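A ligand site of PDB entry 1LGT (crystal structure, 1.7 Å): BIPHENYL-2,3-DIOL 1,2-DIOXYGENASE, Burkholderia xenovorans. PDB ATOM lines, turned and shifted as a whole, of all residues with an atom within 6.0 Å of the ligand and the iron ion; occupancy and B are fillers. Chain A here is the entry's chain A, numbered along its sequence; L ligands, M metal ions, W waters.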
ATOM      1  N   HIS A 145      -0.815   4.937  -6.086  1.00  0.00           N
ATOM      2  CA  HIS A 145      -1.396   3.950  -6.997  1.00  0.00           C
ATOM      3  C   HIS A 145      -2.242   4.586  -8.085  1.00  0.00           C
ATOM      4  O   HIS A 145      -2.490   5.792  -8.065  1.00  0.00           O
ATOM      5  CB  HIS A 145      -2.257   2.914  -6.234  1.00  0.00           C
ATOM      6  CG  HIS A 145      -3.561   3.450  -5.700  1.00  0.00           C
ATOM      7  ND1 HIS A 145      -3.781   3.684  -4.353  1.00  0.00           N
ATOM      8  CD2 HIS A 145      -4.725   3.769  -6.323  1.00  0.00           C
ATOM      9  CE1 HIS A 145      -5.023   4.106  -4.181  1.00  0.00           C
ATOM     10  NE2 HIS A 145      -5.616   4.168  -5.361  1.00  0.00           N
ATOM     11  N   VAL A 147      -5.555   3.367 -11.053  1.00  0.00           N
ATOM     12  CA  VAL A 147      -6.484   2.340 -11.469  1.00  0.00           C
ATOM     13  C   VAL A 147      -6.542   2.269 -12.976  1.00  0.00           C
ATOM     14  O   VAL A 147      -6.989   3.198 -13.653  1.00  0.00           O
ATOM     15  CB  VAL A 147      -7.884   2.619 -10.898  1.00  0.00           C
ATOM     16  CG1 VAL A 147      -8.840   1.487 -11.260  1.00  0.00           C
ATOM     17  CG2 VAL A 147      -7.794   2.791  -9.394  1.00  0.00           C
ATOM     18  N   ILE A 172     -13.159  -6.233  -5.276  1.00  0.00           N
ATOM     19  CA  ILE A 172     -14.380  -5.535  -4.909  1.00  0.00           C
ATOM     20  C   ILE A 172     -15.306  -5.604  -6.099  1.00  0.00           C
ATOM     21  O   ILE A 172     -14.976  -5.138  -7.183  1.00  0.00           O
ATOM     22  CB  ILE A 172     -14.123  -4.045  -4.564  1.00  0.00           C
ATOM     23  CG1 ILE A 172     -13.197  -3.939  -3.354  1.00  0.00           C
ATOM     24  CG2 ILE A 172     -15.457  -3.364  -4.249  1.00  0.00           C
ATOM     25  CD1 ILE A 172     -12.962  -2.522  -2.883  1.00  0.00           C
ATOM     26  N   MET A 174     -17.864  -4.103  -7.851  1.00  0.00           N
ATOM     27  CA  MET A 174     -18.469  -2.777  -7.959  1.00  0.00           C
ATOM     28  C   MET A 174     -19.832  -2.773  -8.623  1.00  0.00           C
ATOM     29  O   MET A 174     -19.964  -3.173  -9.775  1.00  0.00           O
ATOM     30  CB  MET A 174     -17.554  -1.869  -8.779  1.00  0.00           C
ATOM     31  CG  MET A 174     -16.120  -1.800  -8.298  1.00  0.00           C
ATOM     32  SD  MET A 174     -15.912  -0.615  -6.981  1.00  0.00           S
ATOM     33  CE  MET A 174     -14.119  -0.571  -6.836  1.00  0.00           C
ATOM     34  N   ALA A 184     -13.250  -5.273  -9.452  1.00  0.00           N
ATOM     35  CA  ALA A 184     -12.085  -4.414  -9.459  1.00  0.00           C
ATOM     36  C   ALA A 184     -11.033  -5.198  -8.678  1.00  0.00           C
ATOM     37  O   ALA A 184     -11.305  -5.666  -7.572  1.00  0.00           O
ATOM     38  CB  ALA A 184     -12.376  -3.095  -8.761  1.00  0.00           C
ATOM     39  N   PHE A 186      -7.351  -5.360  -6.819  1.00  0.00           N
ATOM     40  CA  PHE A 186      -6.347  -4.499  -6.178  1.00  0.00           C
ATOM     41  C   PHE A 186      -5.087  -5.323  -5.961  1.00  0.00           C
ATOM     42  O   PHE A 186      -5.119  -6.363  -5.306  1.00  0.00           O
ATOM     43  CB  PHE A 186      -6.906  -3.943  -4.864  1.00  0.00           C
ATOM     44  CG  PHE A 186      -8.130  -3.104  -5.069  1.00  0.00           C
ATOM     45  CD1 PHE A 186      -9.382  -3.699  -5.274  1.00  0.00           C
ATOM     46  CD2 PHE A 186      -8.031  -1.716  -5.146  1.00  0.00           C
ATOM     47  CE1 PHE A 186     -10.498  -2.920  -5.572  1.00  0.00           C
ATOM     48  CE2 PHE A 186      -9.150  -0.931  -5.436  1.00  0.00           C
ATOM     49  CZ  PHE A 186     -10.387  -1.537  -5.653  1.00  0.00           C
ATOM     50  N   HIS A 194      -2.345  -1.448  -2.244  1.00  0.00           N
ATOM     51  CA  HIS A 194      -2.343  -1.606  -3.685  1.00  0.00           C
ATOM     52  C   HIS A 194      -1.586  -0.473  -4.362  1.00  0.00           C
ATOM     53  O   HIS A 194      -1.643   0.683  -3.931  1.00  0.00           O
ATOM     54  CB  HIS A 194      -3.765  -1.749  -4.292  1.00  0.00           C
ATOM     55  CG  HIS A 194      -4.694  -0.613  -4.008  1.00  0.00           C
ATOM     56  ND1 HIS A 194      -5.316  -0.441  -2.795  1.00  0.00           N
ATOM     57  CD2 HIS A 194      -5.157   0.381  -4.817  1.00  0.00           C
ATOM     58  CE1 HIS A 194      -6.126   0.601  -2.859  1.00  0.00           C
ATOM     59  NE2 HIS A 194      -6.047   1.121  -4.070  1.00  0.00           N
ATOM     60  N   ALA A 197      -4.680  -1.057  -9.507  1.00  0.00           N
ATOM     61  CA  ALA A 197      -6.006  -1.659  -9.451  1.00  0.00           C
ATOM     62  C   ALA A 197      -6.389  -1.837 -10.916  1.00  0.00           C
ATOM     63  O   ALA A 197      -5.936  -1.065 -11.770  1.00  0.00           O
ATOM     64  CB  ALA A 197      -6.990  -0.737  -8.746  1.00  0.00           C
ATOM     65  N   ALA A 199      -9.821  -2.657 -13.523  1.00  0.00           N
ATOM     66  CA  ALA A 199     -11.274  -2.777 -13.635  1.00  0.00           C
ATOM     67  C   ALA A 199     -11.754  -2.424 -15.029  1.00  0.00           C
ATOM     68  O   ALA A 199     -11.128  -1.635 -15.738  1.00  0.00           O
ATOM     69  CB  ALA A 199     -11.949  -1.870 -12.603  1.00  0.00           C
ATOM     70  N   PHE A 201     -14.093  -0.428 -16.404  1.00  0.00           N
ATOM     71  CA  PHE A 201     -15.000   0.701 -16.267  1.00  0.00           C
ATOM     72  C   PHE A 201     -15.247   1.353 -17.623  1.00  0.00           C
ATOM     73  O   PHE A 201     -14.371   1.365 -18.481  1.00  0.00           O
ATOM     74  CB  PHE A 201     -14.439   1.771 -15.330  1.00  0.00           C
ATOM     75  CG  PHE A 201     -14.274   1.320 -13.900  1.00  0.00           C
ATOM     76  CD1 PHE A 201     -15.237   0.534 -13.294  1.00  0.00           C
ATOM     77  CD2 PHE A 201     -13.159   1.723 -13.164  1.00  0.00           C
ATOM     78  CE1 PHE A 201     -15.105   0.153 -11.947  1.00  0.00           C
ATOM     79  CE2 PHE A 201     -13.029   1.350 -11.824  1.00  0.00           C
ATOM     80  CZ  PHE A 201     -14.000   0.561 -11.220  1.00  0.00           C
ATOM     81  N   HIS A 208      -8.710   5.592 -14.266  1.00  0.00           N
ATOM     82  CA  HIS A 208      -9.831   6.302 -13.672  1.00  0.00           C
ATOM     83  C   HIS A 208      -9.246   7.384 -12.782  1.00  0.00           C
ATOM     84  O   HIS A 208      -9.716   8.524 -12.771  1.00  0.00           O
ATOM     85  CB  HIS A 208     -10.694   5.340 -12.852  1.00  0.00           C
ATOM     86  CG  HIS A 208     -11.695   6.033 -11.977  1.00  0.00           C
ATOM     87  ND1 HIS A 208     -11.429   6.385 -10.672  1.00  0.00           N
ATOM     88  CD2 HIS A 208     -12.946   6.489 -12.242  1.00  0.00           C
ATOM     89  CE1 HIS A 208     -12.462   7.024 -10.165  1.00  0.00           C
ATOM     90  NE2 HIS A 208     -13.401   7.104 -11.100  1.00  0.00           N
ATOM     91  N   HIS A 209      -8.217   7.034 -12.026  1.00  0.00           N
ATOM     92  CA  HIS A 209      -7.563   7.992 -11.148  1.00  0.00           C
ATOM     93  C   HIS A 209      -6.189   7.515 -10.702  1.00  0.00           C
ATOM     94  O   HIS A 209      -5.843   6.344 -10.887  1.00  0.00           O
ATOM     95  CB  HIS A 209      -8.397   8.254  -9.878  1.00  0.00           C
ATOM     96  CG  HIS A 209      -8.419   7.110  -8.907  1.00  0.00           C
ATOM     97  ND1 HIS A 209      -9.343   6.086  -8.987  1.00  0.00           N
ATOM     98  CD2 HIS A 209      -7.673   6.852  -7.798  1.00  0.00           C
ATOM     99  CE1 HIS A 209      -9.167   5.251  -7.969  1.00  0.00           C
ATOM    100  NE2 HIS A 209      -8.163   5.696  -7.241  1.00  0.00           N
ATOM    101  N   MET A 211      -3.555   8.073  -7.204  1.00  0.00           N
ATOM    102  CA  MET A 211      -3.726   8.434  -5.808  1.00  0.00           C
ATOM    103  C   MET A 211      -2.414   8.838  -5.152  1.00  0.00           C
ATOM    104  O   MET A 211      -1.374   8.251  -5.415  1.00  0.00           O
ATOM    105  CB  MET A 211      -4.328   7.241  -5.045  1.00  0.00           C
ATOM    106  CG  MET A 211      -4.645   7.460  -3.569  1.00  0.00           C
ATOM    107  SD  MET A 211      -3.245   7.298  -2.421  1.00  0.00           S
ATOM    108  CE  MET A 211      -2.434   5.897  -3.034  1.00  0.00           C
ATOM    109  N   HIS A 240     -12.138   3.681   2.678  1.00  0.00           N
ATOM    110  CA  HIS A 240     -12.311   2.476   1.894  1.00  0.00           C
ATOM    111  C   HIS A 240     -12.404   1.206   2.734  1.00  0.00           C
ATOM    112  O   HIS A 240     -11.833   1.115   3.819  1.00  0.00           O
ATOM    113  CB  HIS A 240     -11.158   2.330   0.896  1.00  0.00           C
ATOM    114  CG  HIS A 240     -11.236   3.282  -0.252  1.00  0.00           C
ATOM    115  ND1 HIS A 240     -12.311   3.323  -1.120  1.00  0.00           N
ATOM    116  CD2 HIS A 240     -10.359   4.222  -0.692  1.00  0.00           C
ATOM    117  CE1 HIS A 240     -12.096   4.247  -2.036  1.00  0.00           C
ATOM    118  NE2 HIS A 240     -10.914   4.807  -1.804  1.00  0.00           N
ATOM    119  N   THR A 241     -13.134   0.230   2.217  1.00  0.00           N
ATOM    120  CA  THR A 241     -13.315  -1.048   2.888  1.00  0.00           C
ATOM    121  C   THR A 241     -12.079  -1.943   2.859  1.00  0.00           C
ATOM    122  O   THR A 241     -11.837  -2.703   3.808  1.00  0.00           O
ATOM    123  CB  THR A 241     -14.453  -1.843   2.221  1.00  0.00           C
ATOM    124  OG1 THR A 241     -14.222  -1.876   0.804  1.00  0.00           O
ATOM    125  CG2 THR A 241     -15.801  -1.223   2.506  1.00  0.00           C
ATOM    126  N   ASN A 242     -11.283  -1.852   1.790  1.00  0.00           N
ATOM    127  CA  ASN A 242     -10.122  -2.721   1.666  1.00  0.00           C
ATOM    128  C   ASN A 242      -8.800  -2.196   2.216  1.00  0.00           C
ATOM    129  O   ASN A 242      -8.163  -2.881   3.018  1.00  0.00           O
ATOM    130  CB  ASN A 242      -9.961  -3.195   0.205  1.00  0.00           C
ATOM    131  CG  ASN A 242      -9.791  -2.051  -0.789  1.00  0.00           C
ATOM    132  OD1 ASN A 242      -9.939  -0.880  -0.463  1.00  0.00           O
ATOM    133  ND2 ASN A 242      -9.467  -2.406  -2.035  1.00  0.00           N
ATOM    134  N   ASP A 243      -8.357  -1.009   1.802  1.00  0.00           N
ATOM    135  CA  ASP A 243      -7.106  -0.491   2.349  1.00  0.00           C
ATOM    136  C   ASP A 243      -7.325   0.453   3.530  1.00  0.00           C
ATOM    137  O   ASP A 243      -6.361   0.916   4.152  1.00  0.00           O
ATOM    138  CB  ASP A 243      -6.281   0.188   1.247  1.00  0.00           C
ATOM    139  CG  ASP A 243      -6.843   1.520   0.809  1.00  0.00           C
ATOM    140  OD1 ASP A 243      -7.993   1.835   1.151  1.00  0.00           O
ATOM    141  OD2 ASP A 243      -6.111   2.244   0.100  1.00  0.00           O
ATOM    142  N   MET A 245      -8.193   3.465   3.667  1.00  0.00           N
ATOM    143  CA  MET A 245      -7.690   4.815   3.474  1.00  0.00           C
ATOM    144  C   MET A 245      -8.831   5.809   3.565  1.00  0.00           C
ATOM    145  O   MET A 245      -9.936   5.553   3.066  1.00  0.00           O
ATOM    146  CB  MET A 245      -7.017   4.951   2.110  1.00  0.00           C
ATOM    147  CG  MET A 245      -6.553   6.362   1.812  1.00  0.00           C
ATOM    148  SD  MET A 245      -5.726   6.486   0.233  1.00  0.00           S
ATOM    149  CE  MET A 245      -4.198   5.568   0.594  1.00  0.00           C
ATOM    150  N   TYR A 249     -12.084  12.299  -3.720  1.00  0.00           N
ATOM    151  CA  TYR A 249     -11.681  12.272  -5.128  1.00  0.00           C
ATOM    152  C   TYR A 249     -12.026  13.620  -5.743  1.00  0.00           C
ATOM    153  O   TYR A 249     -12.955  14.293  -5.294  1.00  0.00           O
ATOM    154  CB  TYR A 249     -12.424  11.170  -5.890  1.00  0.00           C
ATOM    155  CG  TYR A 249     -12.078   9.751  -5.482  1.00  0.00           C
ATOM    156  CD1 TYR A 249     -12.564   9.222  -4.298  1.00  0.00           C
ATOM    157  CD2 TYR A 249     -11.296   8.937  -6.308  1.00  0.00           C
ATOM    158  CE1 TYR A 249     -12.292   7.901  -3.943  1.00  0.00           C
ATOM    159  CE2 TYR A 249     -11.013   7.619  -5.965  1.00  0.00           C
ATOM    160  CZ  TYR A 249     -11.523   7.113  -4.785  1.00  0.00           C
ATOM    161  OH  TYR A 249     -11.282   5.808  -4.455  1.00  0.00           O
ATOM    162  N   GLU A 259      -7.131  10.842  -6.323  1.00  0.00           N
ATOM    163  CA  GLU A 259      -7.608  10.483  -5.002  1.00  0.00           C
ATOM    164  C   GLU A 259      -6.525  11.009  -4.064  1.00  0.00           C
ATOM    165  O   GLU A 259      -5.335  10.869  -4.351  1.00  0.00           O
ATOM    166  CB  GLU A 259      -7.751   8.973  -4.875  1.00  0.00           C
ATOM    167  CG  GLU A 259      -8.182   8.540  -3.476  1.00  0.00           C
ATOM    168  CD  GLU A 259      -8.396   7.043  -3.373  1.00  0.00           C
ATOM    169  OE1 GLU A 259      -7.899   6.294  -4.245  1.00  0.00           O
ATOM    170  OE2 GLU A 259      -9.067   6.614  -2.414  1.00  0.00           O
ATOM    171  N   PRO A 279     -17.029  -0.472  -2.010  1.00  0.00           N
ATOM    172  CA  PRO A 279     -15.678   0.095  -1.963  1.00  0.00           C
ATOM    173  C   PRO A 279     -15.464   1.025  -0.766  1.00  0.00           C
ATOM    174  O   PRO A 279     -14.325   1.398  -0.462  1.00  0.00           O
ATOM    175  CB  PRO A 279     -15.576   0.833  -3.286  1.00  0.00           C
ATOM    176  CG  PRO A 279     -16.961   1.404  -3.419  1.00  0.00           C
ATOM    177  CD  PRO A 279     -17.842   0.209  -3.029  1.00  0.00           C
ATOM    178  N   SER A 280     -16.540   1.415  -0.093  1.00  0.00           N
ATOM    179  CA  SER A 280     -16.419   2.346   1.027  1.00  0.00           C
ATOM    180  C   SER A 280     -17.178   1.944   2.295  1.00  0.00           C
ATOM    181  O   SER A 280     -18.347   1.551   2.236  1.00  0.00           O
ATOM    182  CB  SER A 280     -16.868   3.736   0.583  1.00  0.00           C
ATOM    183  OG  SER A 280     -16.123   4.168  -0.544  1.00  0.00           O
HETATM  184  C1  LIG L   1     -11.545   2.294  -4.909  1.00  0.00           C
HETATM  185  C2  LIG L   1     -10.283   2.904  -4.732  1.00  0.00           C
HETATM  186  O1  LIG L   1      -9.851   3.910  -5.553  1.00  0.00           O
HETATM  187  C3  LIG L   1      -9.415   2.495  -3.691  1.00  0.00           C
HETATM  188  O2  LIG L   1      -8.181   3.120  -3.553  1.00  0.00           O
HETATM  189  C4  LIG L   1      -9.788   1.459  -2.804  1.00  0.00           C
HETATM  190  C5  LIG L   1     -11.060   0.840  -2.976  1.00  0.00           C
HETATM  191  C6  LIG L   1     -11.928   1.256  -4.023  1.00  0.00           C
HETATM  192  C7  LIG L   1     -12.451   2.736  -6.026  1.00  0.00           C
HETATM  193  C8  LIG L   1     -12.158   2.458  -7.391  1.00  0.00           C
HETATM  194  C9  LIG L   1     -13.022   2.896  -8.431  1.00  0.00           C
HETATM  195  C10 LIG L   1     -14.199   3.616  -8.116  1.00  0.00           C
HETATM  196  C11 LIG L   1     -14.503   3.899  -6.759  1.00  0.00           C
HETATM  197  C12 LIG L   1     -13.627   3.463  -5.732  1.00  0.00           C
HETATM  198 CL1  LIG L   1     -10.742   1.577  -7.930  1.00  0.00          CL
HETATM  199 FE    FE M   1      -7.892   4.539  -5.302  1.00  0.00          FE
HETATM  200  O   HOH W   1      -6.836   4.436  -1.332  1.00  0.00           O
HETATM  201  O   HOH W   2      -7.588   2.435  -6.518  1.00  0.00           O
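O1 of the ligand sits close to OH of Tyr 249 (2.6 Å).
NE2 of His 194 sits close to O2 of the ligand (3.0 Å).
Tyr 249 touches the iron ion.
Within 4 Å of the iron ion: His 145, His 209, Tyr 249 and Glu 259.
Residues that only touch the ligand: Val 147 (3.5 Å), Ile 172 (3.9 Å), Met 174 (3.7 Å), Phe 186 (3.6 Å), Phe 201 (3.7 Å), His 240 (3.3 Å), Asn 242 (3.2 Å) and Pro 279 (3.7 Å).
Hydrophobic or aromatic side chains that line the ligand: His 145, Val 147, Ile 172, Met 174, Phe 186, His 194, Phe 201, His 209, His 240, Tyr 249 and Pro 279.
OE2 of Glu 259 is in hydrogen-bond range of NE2 of His 240 (2.7 Å).
The backbone carbonyl oxygen of His 209 sits at hydrogen-bond distance from the backbone NH of Val 147, 3.0 Å away.
A ring nitrogen (ND1) of His 145 sits close to a ring nitrogen (NE2) of His 194 (3.4 Å).
The backbone carbonyl oxygen (O) of His 145 sits at hydrogen-bond distance from the backbone NH (N) of Met 211.
OH of Tyr 249 is in hydrogen-bond range of NE2 of His 240 (2.9 Å).
The backbone NH (N) of His 240 is in hydrogen-bond range of the backbone carbonyl oxygen (O) of Met 245 (2.9 Å).
O of Val 147 sits at hydrogen-bond distance from N of His 208, 3.0 Å away.
N of Ala 184 is in hydrogen-bond range of O of Ile 172, 2.9 Å away.
The iron ion is bound by OE1 of Glu 259 (2.0 Å), O1 of the ligand (2.1 Å), O2 of the ligand (2.3 Å), NE2 of His 209 (2.3 Å), NE2 of His 145 (2.3 Å) and water W2 (2.4 Å).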
